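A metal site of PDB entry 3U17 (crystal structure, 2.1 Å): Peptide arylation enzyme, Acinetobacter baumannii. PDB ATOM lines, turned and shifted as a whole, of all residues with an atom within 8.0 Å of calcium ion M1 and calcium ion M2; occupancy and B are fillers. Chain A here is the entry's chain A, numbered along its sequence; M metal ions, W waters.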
ATOM      1  N   VAL A 282     -17.359  15.280  14.124  1.00  0.00           N
ATOM      2  CA  VAL A 282     -18.104  14.916  12.916  1.00  0.00           C
ATOM      3  C   VAL A 282     -18.716  13.524  13.075  1.00  0.00           C
ATOM      4  O   VAL A 282     -18.041  12.587  13.523  1.00  0.00           O
ATOM      5  CB  VAL A 282     -17.157  14.921  11.690  1.00  0.00           C
ATOM      6  CG1 VAL A 282     -17.818  14.236  10.492  1.00  0.00           C
ATOM      7  CG2 VAL A 282     -16.719  16.340  11.358  1.00  0.00           C
ATOM      8  N   ASN A 283     -19.990  13.375  12.705  1.00  0.00           N
ATOM      9  CA  ASN A 283     -20.643  12.088  12.843  1.00  0.00           C
ATOM     10  C   ASN A 283     -21.109  11.487  11.515  1.00  0.00           C
ATOM     11  O   ASN A 283     -21.687  10.416  11.470  1.00  0.00           O
ATOM     12  CB  ASN A 283     -21.773  12.147  13.874  1.00  0.00           C
ATOM     13  CG  ASN A 283     -22.762  13.283  13.597  1.00  0.00           C
ATOM     14  OD1 ASN A 283     -22.909  13.750  12.462  1.00  0.00           O
ATOM     15  ND2 ASN A 283     -23.464  13.713  14.634  1.00  0.00           N
ATOM     16  N   LYS A 303      -7.743   5.349  15.314  1.00  0.00           N
ATOM     17  CA  LYS A 303      -9.059   4.920  15.780  1.00  0.00           C
ATOM     18  C   LYS A 303      -9.724   5.988  16.637  1.00  0.00           C
ATOM     19  O   LYS A 303     -10.883   6.347  16.410  1.00  0.00           O
ATOM     20  CB  LYS A 303      -8.886   3.646  16.606  1.00  0.00           C
ATOM     21  CG  LYS A 303      -9.924   2.585  16.337  1.00  0.00           C
ATOM     22  CD  LYS A 303      -9.550   1.295  17.065  1.00  0.00           C
ATOM     23  CE  LYS A 303      -9.208   1.602  18.514  1.00  0.00           C
ATOM     24  NZ  LYS A 303     -10.273   2.440  19.155  1.00  0.00           N
ATOM     25  N   ILE A 306     -11.432   9.131  14.919  1.00  0.00           N
ATOM     26  CA  ILE A 306     -12.627   8.979  14.098  1.00  0.00           C
ATOM     27  C   ILE A 306     -13.760   8.239  14.778  1.00  0.00           C
ATOM     28  O   ILE A 306     -14.734   7.864  14.128  1.00  0.00           O
ATOM     29  CB  ILE A 306     -12.298   8.281  12.762  1.00  0.00           C
ATOM     30  CG1 ILE A 306     -11.932   6.817  13.004  1.00  0.00           C
ATOM     31  CG2 ILE A 306     -11.167   9.000  12.050  1.00  0.00           C
ATOM     32  CD1 ILE A 306     -11.887   6.020  11.734  1.00  0.00           C
ATOM     33  N   GLN A 307     -13.661   7.994  16.084  1.00  0.00           N
ATOM     34  CA  GLN A 307     -14.728   7.254  16.755  1.00  0.00           C
ATOM     35  C   GLN A 307     -16.112   7.912  16.603  1.00  0.00           C
ATOM     36  O   GLN A 307     -17.119   7.223  16.619  1.00  0.00           O
ATOM     37  CB  GLN A 307     -14.381   6.991  18.221  1.00  0.00           C
ATOM     38  CG  GLN A 307     -13.341   5.877  18.412  1.00  0.00           C
ATOM     39  CD  GLN A 307     -13.773   4.560  17.789  1.00  0.00           C
ATOM     40  OE1 GLN A 307     -14.516   3.798  18.397  1.00  0.00           O
ATOM     41  NE2 GLN A 307     -13.312   4.295  16.561  1.00  0.00           N
ATOM     42  N   SER A 308     -16.144   9.235  16.436  1.00  0.00           N
ATOM     43  CA  SER A 308     -17.454   9.906  16.308  1.00  0.00           C
ATOM     44  C   SER A 308     -18.246   9.620  15.021  1.00  0.00           C
ATOM     45  O   SER A 308     -19.452   9.828  14.979  1.00  0.00           O
ATOM     46  CB  SER A 308     -17.334  11.428  16.555  1.00  0.00           C
ATOM     47  OG  SER A 308     -16.465  12.051  15.633  1.00  0.00           O
ATOM     48  N   LEU A 309     -17.581   9.128  13.967  1.00  0.00           N
ATOM     49  CA  LEU A 309     -18.300   8.808  12.730  1.00  0.00           C
ATOM     50  C   LEU A 309     -19.442   7.855  13.023  1.00  0.00           C
ATOM     51  O   LEU A 309     -19.238   6.839  13.655  1.00  0.00           O
ATOM     52  CB  LEU A 309     -17.376   8.176  11.690  1.00  0.00           C
ATOM     53  CG  LEU A 309     -16.353   9.081  11.021  1.00  0.00           C
ATOM     54  CD1 LEU A 309     -15.581   8.326   9.952  1.00  0.00           C
ATOM     55  CD2 LEU A 309     -17.047  10.327  10.424  1.00  0.00           C
ATOM     56  N   LYS A 310     -20.649   8.152  12.547  1.00  0.00           N
ATOM     57  CA  LYS A 310     -21.759   7.230  12.739  1.00  0.00           C
ATOM     58  C   LYS A 310     -22.226   6.658  11.412  1.00  0.00           C
ATOM     59  O   LYS A 310     -22.815   5.573  11.357  1.00  0.00           O
ATOM     60  CB  LYS A 310     -22.946   7.939  13.408  1.00  0.00           C
ATOM     61  CG  LYS A 310     -22.770   8.284  14.886  1.00  0.00           C
ATOM     62  CD  LYS A 310     -24.067   8.913  15.399  1.00  0.00           C
ATOM     63  CE  LYS A 310     -23.953   9.459  16.806  1.00  0.00           C
ATOM     64  NZ  LYS A 310     -25.261  10.068  17.238  1.00  0.00           N
ATOM     65  N   LEU A 311     -22.010   7.408  10.338  1.00  0.00           N
ATOM     66  CA  LEU A 311     -22.506   7.005   9.031  1.00  0.00           C
ATOM     67  C   LEU A 311     -21.526   7.469   7.964  1.00  0.00           C
ATOM     68  O   LEU A 311     -21.104   8.631   7.971  1.00  0.00           O
ATOM     69  CB  LEU A 311     -23.902   7.593   8.766  1.00  0.00           C
ATOM     70  CG  LEU A 311     -24.526   7.360   7.383  1.00  0.00           C
ATOM     71  CD1 LEU A 311     -24.668   5.870   7.094  1.00  0.00           C
ATOM     72  CD2 LEU A 311     -25.889   8.105   7.228  1.00  0.00           C
ATOM     73  N   GLN A 326     -15.243  -3.729   5.165  1.00  0.00           N
ATOM     74  CA  GLN A 326     -14.219  -3.108   5.988  1.00  0.00           C
ATOM     75  C   GLN A 326     -14.659  -1.788   6.610  1.00  0.00           C
ATOM     76  O   GLN A 326     -14.045  -1.336   7.571  1.00  0.00           O
ATOM     77  CB  GLN A 326     -12.941  -2.907   5.188  1.00  0.00           C
ATOM     78  CG  GLN A 326     -12.253  -4.208   4.798  1.00  0.00           C
ATOM     79  CD  GLN A 326     -10.873  -3.960   4.229  1.00  0.00           C
ATOM     80  OE1 GLN A 326      -9.968  -3.477   4.928  1.00  0.00           O
ATOM     81  NE2 GLN A 326     -10.698  -4.293   2.941  1.00  0.00           N
ATOM     82  N   VAL A 327     -15.707  -1.165   6.073  1.00  0.00           N
ATOM     83  CA  VAL A 327     -16.132   0.148   6.583  1.00  0.00           C
ATOM     84  C   VAL A 327     -16.592   0.073   8.045  1.00  0.00           C
ATOM     85  O   VAL A 327     -16.015   0.725   8.909  1.00  0.00           O
ATOM     86  CB  VAL A 327     -17.184   0.814   5.661  1.00  0.00           C
ATOM     87  CG1 VAL A 327     -17.889   1.964   6.385  1.00  0.00           C
ATOM     88  CG2 VAL A 327     -16.533   1.302   4.370  1.00  0.00           C
ATOM     89  N   PRO A 328     -17.624  -0.733   8.336  1.00  0.00           N
ATOM     90  CA  PRO A 328     -18.036  -0.879   9.743  1.00  0.00           C
ATOM     91  C   PRO A 328     -16.957  -1.567  10.564  1.00  0.00           C
ATOM     92  O   PRO A 328     -16.811  -1.297  11.749  1.00  0.00           O
ATOM     93  CB  PRO A 328     -19.266  -1.779   9.667  1.00  0.00           C
ATOM     94  CG  PRO A 328     -19.158  -2.474   8.347  1.00  0.00           C
ATOM     95  CD  PRO A 328     -18.484  -1.508   7.425  1.00  0.00           C
ATOM     96  N   GLU A 329     -16.198  -2.459   9.929  1.00  0.00           N
ATOM     97  CA  GLU A 329     -15.165  -3.195  10.644  1.00  0.00           C
ATOM     98  C   GLU A 329     -14.010  -2.307  11.086  1.00  0.00           C
ATOM     99  O   GLU A 329     -13.534  -2.413  12.208  1.00  0.00           O
ATOM    100  CB  GLU A 329     -14.616  -4.311   9.756  1.00  0.00           C
ATOM    101  CG  GLU A 329     -13.550  -5.154  10.420  1.00  0.00           C
ATOM    102  CD  GLU A 329     -14.128  -6.090  11.460  1.00  0.00           C
ATOM    103  OE1 GLU A 329     -15.215  -6.679  11.197  1.00  0.00           O
ATOM    104  OE2 GLU A 329     -13.502  -6.253  12.537  1.00  0.00           O
ATOM    105  N   VAL A 330     -13.545  -1.431  10.196  1.00  0.00           N
ATOM    106  CA  VAL A 330     -12.345  -0.642  10.502  1.00  0.00           C
ATOM    107  C   VAL A 330     -12.659   0.835  10.823  1.00  0.00           C
ATOM    108  O   VAL A 330     -12.064   1.417  11.725  1.00  0.00           O
ATOM    109  CB  VAL A 330     -11.311  -0.731   9.353  1.00  0.00           C
ATOM    110  CG1 VAL A 330     -10.147   0.244   9.582  1.00  0.00           C
ATOM    111  CG2 VAL A 330     -10.783  -2.187   9.217  1.00  0.00           C
ATOM    112  N   LEU A 331     -13.602   1.428  10.088  1.00  0.00           N
ATOM    113  CA  LEU A 331     -13.945   2.831  10.299  1.00  0.00           C
ATOM    114  C   LEU A 331     -14.981   2.976  11.412  1.00  0.00           C
ATOM    115  O   LEU A 331     -15.299   4.083  11.849  1.00  0.00           O
ATOM    116  CB  LEU A 331     -14.426   3.493   8.994  1.00  0.00           C
ATOM    117  CG  LEU A 331     -13.400   3.520   7.853  1.00  0.00           C
ATOM    118  CD1 LEU A 331     -13.938   4.164   6.576  1.00  0.00           C
ATOM    119  CD2 LEU A 331     -12.132   4.232   8.317  1.00  0.00           C
ATOM    120  N   ASN A 332     -15.516   1.840  11.863  1.00  0.00           N
ATOM    121  CA  ASN A 332     -16.349   1.829  13.052  1.00  0.00           C
ATOM    122  C   ASN A 332     -17.618   2.672  12.904  1.00  0.00           C
ATOM    123  O   ASN A 332     -18.033   3.342  13.818  1.00  0.00           O
ATOM    124  CB  ASN A 332     -15.534   2.280  14.287  1.00  0.00           C
ATOM    125  CG  ASN A 332     -14.326   1.372  14.534  1.00  0.00           C
ATOM    126  OD1 ASN A 332     -14.212   0.348  13.900  1.00  0.00           O
ATOM    127  ND2 ASN A 332     -13.429   1.768  15.425  1.00  0.00           N
ATOM    128  N   CYS A 333     -18.238   2.602  11.737  1.00  0.00           N
ATOM    129  CA  CYS A 333     -19.465   3.333  11.515  1.00  0.00           C
ATOM    130  C   CYS A 333     -20.337   2.554  10.540  1.00  0.00           C
ATOM    131  O   CYS A 333     -19.851   1.673   9.824  1.00  0.00           O
ATOM    132  CB  CYS A 333     -19.168   4.736  10.950  1.00  0.00           C
ATOM    133  SG  CYS A 333     -18.226   4.661   9.391  1.00  0.00           S
ATOM    134  N   LYS A 334     -21.609   2.886  10.499  1.00  0.00           N
ATOM    135  CA  LYS A 334     -22.540   2.305   9.556  1.00  0.00           C
ATOM    136  C   LYS A 334     -22.146   2.678   8.118  1.00  0.00           C
ATOM    137  O   LYS A 334     -21.613   3.763   7.864  1.00  0.00           O
ATOM    138  CB  LYS A 334     -23.958   2.820   9.873  1.00  0.00           C
ATOM    139  CG  LYS A 334     -24.997   2.582   8.793  1.00  0.00           C
ATOM    140  CD  LYS A 334     -25.441   1.125   8.752  1.00  0.00           C
ATOM    141  CE  LYS A 334     -26.930   1.010   9.090  1.00  0.00           C
ATOM    142  NZ  LYS A 334     -27.327  -0.434   9.084  1.00  0.00           N
HETATM  143 CA    CA M   1     -18.179   5.360  15.245  1.00  0.00          CA
HETATM  144 CA    CA M   2     -14.033  -2.020  14.617  1.00  0.00          CA
HETATM  145  O   HOH W   1     -11.332  -0.461  14.964  1.00  0.00           O
HETATM  146  O   HOH W   2     -16.606  -2.427  14.455  1.00  0.00           O
HETATM  147  O   HOH W   3     -17.332   3.915  17.107  1.00  0.00           O
HETATM  148  O   HOH W   4     -14.346  -4.508  15.539  1.00  0.00           O
HETATM  149  O   HOH W   5     -16.143   5.556  13.792  1.00  0.00           O
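Calcium ion M2 is bound by OD1 of Asn 332, O of Glu 329, water W2 and water W4.
Slightly farther from calcium ion M2 lies water W1 (3.1 Å).
OD1 of Asn 332 lies close to O of Val 330 (3.2 Å).
The backbone carbonyl oxygen (O) of Val 327 sits at hydrogen-bond distance from the backbone NH (N) of Asn 332 (3.2 Å).
The side-chain amide nitrogen of Gln 307 lies within hydrogen-bond range of the backbone carbonyl oxygen of Lys 303, 3.2 Å away.
Water W5 lies within hydrogen-bond range of the backbone carbonyl oxygen (O) of Leu 331 (2.6 Å) and the backbone carbonyl oxygen (O) of Ile 306 (2.7 Å).
Two residues have an atom within 4 Å of calcium ion M2: Glu 329 and Asn 332.
The nearest printed residue that does not touch calcium ion M2 is Pro 328 (4.1 Å).
Within 4 Å of calcium ion M1: Gln 307, Leu 309 and Asn 332.
Calcium ion M1 is bound by O of Leu 309 (2.4 Å), O of Asn 332 (2.5 Å), water W3 (2.5 Å), water W5 (2.5 Å) and O of Gln 307 (2.5 Å).
Calcium ion M1 has five donor atoms within binding distance.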
